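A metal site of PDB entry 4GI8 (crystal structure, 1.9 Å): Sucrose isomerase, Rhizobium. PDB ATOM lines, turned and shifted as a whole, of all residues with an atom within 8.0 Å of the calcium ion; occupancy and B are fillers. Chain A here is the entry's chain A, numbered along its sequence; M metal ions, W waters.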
ATOM      1  N   PRO A  17     -29.960 -29.891   7.863  1.00  0.00           N
ATOM      2  CA  PRO A  17     -29.000 -28.823   7.506  1.00  0.00           C
ATOM      3  C   PRO A  17     -28.483 -28.846   6.067  1.00  0.00           C
ATOM      4  O   PRO A  17     -28.287 -27.771   5.466  1.00  0.00           O
ATOM      5  CB  PRO A  17     -27.837 -29.049   8.483  1.00  0.00           C
ATOM      6  CG  PRO A  17     -28.461 -29.788   9.617  1.00  0.00           C
ATOM      7  CD  PRO A  17     -29.474 -30.700   9.001  1.00  0.00           C
ATOM      8  N   ARG A  18     -28.291 -30.034   5.525  1.00  0.00           N
ATOM      9  CA  ARG A  18     -27.910 -30.264   4.127  1.00  0.00           C
ATOM     10  C   ARG A  18     -28.763 -29.433   3.127  1.00  0.00           C
ATOM     11  O   ARG A  18     -28.284 -29.011   2.049  1.00  0.00           O
ATOM     12  CB  ARG A  18     -28.107 -31.762   3.858  1.00  0.00           C
ATOM     13  CG  ARG A  18     -27.580 -32.257   2.540  1.00  0.00           C
ATOM     14  CD  ARG A  18     -27.551 -33.797   2.457  1.00  0.00           C
ATOM     15  NE  ARG A  18     -26.967 -34.099   1.166  1.00  0.00           N
ATOM     16  CZ  ARG A  18     -25.681 -34.349   0.953  1.00  0.00           C
ATOM     17  NH1 ARG A  18     -24.813 -34.449   1.971  1.00  0.00           N
ATOM     18  NH2 ARG A  18     -25.265 -34.559  -0.287  1.00  0.00           N
ATOM     19  N   LYS A  21     -29.657 -23.939   4.322  1.00  0.00           N
ATOM     20  CA  LYS A  21     -29.011 -22.752   3.687  1.00  0.00           C
ATOM     21  C   LYS A  21     -27.512 -22.942   3.468  1.00  0.00           C
ATOM     22  O   LYS A  21     -26.782 -23.208   4.428  1.00  0.00           O
ATOM     23  CB  LYS A  21     -29.279 -21.470   4.490  1.00  0.00           C
ATOM     24  CG  LYS A  21     -28.667 -20.176   3.912  1.00  0.00           C
ATOM     25  CD  LYS A  21     -29.391 -19.727   2.641  1.00  0.00           C
ATOM     26  CE  LYS A  21     -28.898 -18.379   2.148  1.00  0.00           C
ATOM     27  NZ  LYS A  21     -27.431 -18.460   1.942  1.00  0.00           N
ATOM     28  N   ASP A  22     -27.087 -22.832   2.209  1.00  0.00           N
ATOM     29  CA  ASP A  22     -25.672 -22.944   1.808  1.00  0.00           C
ATOM     30  C   ASP A  22     -25.059 -21.545   1.818  1.00  0.00           C
ATOM     31  O   ASP A  22     -25.678 -20.597   1.337  1.00  0.00           O
ATOM     32  CB  ASP A  22     -25.591 -23.448   0.369  1.00  0.00           C
ATOM     33  CG  ASP A  22     -24.154 -23.638  -0.140  1.00  0.00           C
ATOM     34  OD1 ASP A  22     -23.165 -23.670   0.638  1.00  0.00           O
ATOM     35  OD2 ASP A  22     -24.048 -23.843  -1.364  1.00  0.00           O
ATOM     36  N   THR A  23     -23.840 -21.424   2.341  1.00  0.00           N
ATOM     37  CA  THR A  23     -23.166 -20.112   2.380  1.00  0.00           C
ATOM     38  C   THR A  23     -21.803 -20.134   1.672  1.00  0.00           C
ATOM     39  O   THR A  23     -21.022 -19.209   1.811  1.00  0.00           O
ATOM     40  CB  THR A  23     -22.956 -19.615   3.833  1.00  0.00           C
ATOM     41  OG1 THR A  23     -22.214 -20.579   4.567  1.00  0.00           O
ATOM     42  CG2 THR A  23     -24.313 -19.323   4.535  1.00  0.00           C
ATOM     43  N   ASN A  24     -21.468 -21.193   0.947  1.00  0.00           N
ATOM     44  CA  ASN A  24     -20.166 -21.218   0.299  1.00  0.00           C
ATOM     45  C   ASN A  24     -20.186 -21.787  -1.128  1.00  0.00           C
ATOM     46  O   ASN A  24     -19.168 -22.227  -1.624  1.00  0.00           O
ATOM     47  CB  ASN A  24     -19.094 -21.898   1.168  1.00  0.00           C
ATOM     48  CG  ASN A  24     -19.231 -23.416   1.158  1.00  0.00           C
ATOM     49  OD1 ASN A  24     -20.329 -23.945   0.990  1.00  0.00           O
ATOM     50  ND2 ASN A  24     -18.127 -24.108   1.303  1.00  0.00           N
ATOM     51  N   GLY A  25     -21.351 -21.814  -1.741  1.00  0.00           N
ATOM     52  CA  GLY A  25     -21.482 -22.238  -3.131  1.00  0.00           C
ATOM     53  C   GLY A  25     -21.300 -23.698  -3.479  1.00  0.00           C
ATOM     54  O   GLY A  25     -21.329 -24.040  -4.653  1.00  0.00           O
ATOM     55  N   ASP A  26     -21.142 -24.601  -2.501  1.00  0.00           N
ATOM     56  CA  ASP A  26     -20.924 -25.990  -2.833  1.00  0.00           C
ATOM     57  C   ASP A  26     -22.233 -26.768  -3.036  1.00  0.00           C
ATOM     58  O   ASP A  26     -22.214 -27.936  -3.348  1.00  0.00           O
ATOM     59  CB  ASP A  26     -19.990 -26.657  -1.827  1.00  0.00           C
ATOM     60  CG  ASP A  26     -20.645 -26.869  -0.456  1.00  0.00           C
ATOM     61  OD1 ASP A  26     -21.791 -26.393  -0.198  1.00  0.00           O
ATOM     62  OD2 ASP A  26     -20.006 -27.549   0.374  1.00  0.00           O
ATOM     63  N   GLY A  27     -23.364 -26.090  -2.896  1.00  0.00           N
ATOM     64  CA  GLY A  27     -24.674 -26.688  -3.133  1.00  0.00           C
ATOM     65  C   GLY A  27     -25.198 -27.513  -1.955  1.00  0.00           C
ATOM     66  O   GLY A  27     -26.244 -28.160  -2.068  1.00  0.00           O
ATOM     67  N   ILE A  28     -24.457 -27.480  -0.839  1.00  0.00           N
ATOM     68  CA  ILE A  28     -24.868 -28.180   0.387  1.00  0.00           C
ATOM     69  C   ILE A  28     -25.052 -27.178   1.549  1.00  0.00           C
ATOM     70  O   ILE A  28     -24.182 -26.360   1.802  1.00  0.00           O
ATOM     71  CB  ILE A  28     -23.846 -29.298   0.769  1.00  0.00           C
ATOM     72  CG1 ILE A  28     -23.788 -30.387  -0.315  1.00  0.00           C
ATOM     73  CG2 ILE A  28     -24.195 -29.927   2.120  1.00  0.00           C
ATOM     74  CD1 ILE A  28     -22.470 -31.168  -0.339  1.00  0.00           C
ATOM     75  N   GLY A  29     -26.174 -27.255   2.272  1.00  0.00           N
ATOM     76  CA  GLY A  29     -26.410 -26.345   3.403  1.00  0.00           C
ATOM     77  C   GLY A  29     -25.401 -26.580   4.503  1.00  0.00           C
ATOM     78  O   GLY A  29     -24.805 -27.645   4.569  1.00  0.00           O
ATOM     79  N   ASP A  30     -25.197 -25.597   5.375  1.00  0.00           N
ATOM     80  CA  ASP A  30     -24.113 -25.687   6.363  1.00  0.00           C
ATOM     81  C   ASP A  30     -24.489 -24.955   7.656  1.00  0.00           C
ATOM     82  O   ASP A  30     -25.556 -24.324   7.736  1.00  0.00           O
ATOM     83  CB  ASP A  30     -22.802 -25.152   5.749  1.00  0.00           C
ATOM     84  CG  ASP A  30     -23.005 -23.862   4.961  1.00  0.00           C
ATOM     85  OD1 ASP A  30     -23.391 -22.834   5.567  1.00  0.00           O
ATOM     86  OD2 ASP A  30     -22.826 -23.863   3.725  1.00  0.00           O
ATOM     87  N   PHE A  31     -23.626 -25.025   8.665  1.00  0.00           N
ATOM     88  CA  PHE A  31     -23.902 -24.389   9.948  1.00  0.00           C
ATOM     89  C   PHE A  31     -23.996 -22.880   9.831  1.00  0.00           C
ATOM     90  O   PHE A  31     -24.870 -22.265  10.448  1.00  0.00           O
ATOM     91  CB  PHE A  31     -22.827 -24.740  10.987  1.00  0.00           C
ATOM     92  CG  PHE A  31     -22.926 -26.141  11.548  1.00  0.00           C
ATOM     93  CD1 PHE A  31     -24.141 -26.709  11.880  1.00  0.00           C
ATOM     94  CD2 PHE A  31     -21.760 -26.880  11.754  1.00  0.00           C
ATOM     95  CE1 PHE A  31     -24.200 -27.988  12.423  1.00  0.00           C
ATOM     96  CE2 PHE A  31     -21.814 -28.169  12.283  1.00  0.00           C
ATOM     97  CZ  PHE A  31     -23.041 -28.698  12.642  1.00  0.00           C
ATOM     98  N   LYS A  32     -23.086 -22.251   9.086  1.00  0.00           N
ATOM     99  CA  LYS A  32     -23.123 -20.780   8.944  1.00  0.00           C
ATOM    100  C   LYS A  32     -24.457 -20.355   8.345  1.00  0.00           C
ATOM    101  O   LYS A  32     -25.047 -19.354   8.757  1.00  0.00           O
ATOM    102  CB  LYS A  32     -21.971 -20.299   8.061  1.00  0.00           C
ATOM    103  CG  LYS A  32     -21.825 -18.771   8.068  1.00  0.00           C
ATOM    104  CD  LYS A  32     -20.641 -18.319   7.204  1.00  0.00           C
ATOM    105  N   GLY A  33     -24.965 -21.160   7.397  1.00  0.00           N
ATOM    106  CA  GLY A  33     -26.285 -20.885   6.838  1.00  0.00           C
ATOM    107  C   GLY A  33     -27.409 -20.915   7.835  1.00  0.00           C
ATOM    108  O   GLY A  33     -28.315 -20.065   7.808  1.00  0.00           O
ATOM    109  N   LYS A  74     -17.678 -32.415   7.783  1.00  0.00           N
ATOM    110  CA  LYS A  74     -16.855 -31.440   7.028  1.00  0.00           C
ATOM    111  C   LYS A  74     -17.688 -30.449   6.215  1.00  0.00           C
ATOM    112  O   LYS A  74     -17.410 -29.255   6.211  1.00  0.00           O
ATOM    113  CB  LYS A  74     -15.874 -32.188   6.092  1.00  0.00           C
ATOM    114  CG  LYS A  74     -14.649 -32.779   6.795  1.00  0.00           C
ATOM    115  N   GLU A  75     -18.715 -30.950   5.514  1.00  0.00           N
ATOM    116  CA  GLU A  75     -19.618 -30.073   4.753  1.00  0.00           C
ATOM    117  C   GLU A  75     -20.345 -28.993   5.607  1.00  0.00           C
ATOM    118  O   GLU A  75     -20.639 -27.901   5.113  1.00  0.00           O
ATOM    119  CB  GLU A  75     -20.663 -30.885   3.976  1.00  0.00           C
ATOM    120  CG  GLU A  75     -20.117 -31.590   2.750  1.00  0.00           C
ATOM    121  CD  GLU A  75     -19.456 -32.924   3.086  1.00  0.00           C
ATOM    122  OE1 GLU A  75     -19.381 -33.322   4.281  1.00  0.00           O
ATOM    123  OE2 GLU A  75     -19.010 -33.596   2.133  1.00  0.00           O
ATOM    124  N   TYR A  76     -20.624 -29.287   6.880  1.00  0.00           N
ATOM    125  CA  TYR A  76     -21.377 -28.308   7.691  1.00  0.00           C
ATOM    126  C   TYR A  76     -20.492 -27.212   8.285  1.00  0.00           C
ATOM    127  O   TYR A  76     -20.975 -26.125   8.551  1.00  0.00           O
ATOM    128  CB  TYR A  76     -22.194 -28.996   8.789  1.00  0.00           C
ATOM    129  CG  TYR A  76     -23.243 -29.949   8.212  1.00  0.00           C
ATOM    130  CD1 TYR A  76     -23.580 -29.902   6.852  1.00  0.00           C
ATOM    131  CD2 TYR A  76     -23.933 -30.849   9.027  1.00  0.00           C
ATOM    132  CE1 TYR A  76     -24.528 -30.761   6.317  1.00  0.00           C
ATOM    133  CE2 TYR A  76     -24.890 -31.698   8.496  1.00  0.00           C
ATOM    134  CZ  TYR A  76     -25.170 -31.659   7.143  1.00  0.00           C
ATOM    135  OH  TYR A  76     -26.122 -32.498   6.599  1.00  0.00           O
ATOM    136  N   GLY A  77     -19.220 -27.506   8.483  1.00  0.00           N
ATOM    137  CA  GLY A  77     -18.289 -26.518   9.046  1.00  0.00           C
ATOM    138  C   GLY A  77     -17.340 -27.174  10.035  1.00  0.00           C
ATOM    139  O   GLY A  77     -16.979 -28.348   9.878  1.00  0.00           O
ATOM    140  N   PHE A 431     -31.230 -20.569  -2.036  1.00  0.00           N
ATOM    141  CA  PHE A 431     -30.612 -21.600  -1.193  1.00  0.00           C
ATOM    142  C   PHE A 431     -29.074 -21.608  -1.377  1.00  0.00           C
ATOM    143  O   PHE A 431     -28.323 -21.743  -0.405  1.00  0.00           O
ATOM    144  CB  PHE A 431     -31.206 -22.985  -1.507  1.00  0.00           C
ATOM    145  CG  PHE A 431     -30.368 -24.133  -1.021  1.00  0.00           C
ATOM    146  CD1 PHE A 431     -30.251 -24.380   0.361  1.00  0.00           C
ATOM    147  CD2 PHE A 431     -29.681 -24.944  -1.915  1.00  0.00           C
ATOM    148  CE1 PHE A 431     -29.477 -25.440   0.808  1.00  0.00           C
ATOM    149  CE2 PHE A 431     -28.890 -26.004  -1.453  1.00  0.00           C
ATOM    150  CZ  PHE A 431     -28.782 -26.242  -0.089  1.00  0.00           C
ATOM    151  N   THR A 432     -28.628 -21.456  -2.634  1.00  0.00           N
ATOM    152  CA  THR A 432     -27.198 -21.589  -2.977  1.00  0.00           C
ATOM    153  C   THR A 432     -26.853 -20.661  -4.154  1.00  0.00           C
ATOM    154  O   THR A 432     -27.735 -20.304  -4.950  1.00  0.00           O
ATOM    155  CB  THR A 432     -26.814 -23.049  -3.337  1.00  0.00           C
ATOM    156  OG1 THR A 432     -25.399 -23.124  -3.509  1.00  0.00           O
ATOM    157  CG2 THR A 432     -27.476 -23.549  -4.602  1.00  0.00           C
HETATM  158 CA    CA M   1     -22.112 -25.216   1.940  1.00  0.00          CA
HETATM  159  O   HOH W   1     -20.187 -25.214   3.705  1.00  0.00           O
HETATM  160  O   HOH W   2     -21.260 -27.206   2.658  1.00  0.00           O
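The side-chain hydroxyl of Thr 23 is in hydrogen-bond range of the side-chain carboxylate of Asp 30 (2.7 Å).
The backbone NH (N) of Asp 22 is in hydrogen-bond range of the backbone carbonyl oxygen (O) of Phe 431 (3.1 Å).
The side-chain carboxylate (OD2) of Asp 22 sits at hydrogen-bond distance from the side-chain hydroxyl (OG1) of Thr 432, at 2.6 Å.
The side-chain carboxylate (OD1) of Asp 30 is in hydrogen-bond range of the backbone NH (N) of Gly 33 (2.9 Å).
The backbone NH of Gly 25 is in hydrogen-bond range of the side-chain carboxylate of Asp 22 (3.4 Å).
OD2 of Asp 22 lies within hydrogen-bond range of N of Gly 27, at 2.8 Å.
The backbone carbonyl oxygen (O) of Lys 21 is in hydrogen-bond range of the backbone NH (N) of Asp 30 (3.0 Å).
Within 4 Å of the calcium ion: Asp 22, Asn 24, Asp 26, Ile 28 and Asp 30.
Along chain A the residues within 4 Å of the calcium ion span positions 22 to 30.
The nearest printed residue that does not touch the calcium ion is Thr 23 (4.2 Å).
The calcium ion is bound by OD1 of Asp 22 (2.3 Å), water W2 (2.3 Å), OD2 of Asp 30 (2.4 Å), O of Ile 28 (2.4 Å), OD1 of Asn 24 (2.4 Å), OD1 of Asp 26 (2.5 Å) and water W1 (2.6 Å).
Water W1 bridges O of Glu 75 (3.1 Å) and ND2 of Asn 24 (3.4 Å).
Water W2 bridges O of Glu 75 and OD2 of Asp 26.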
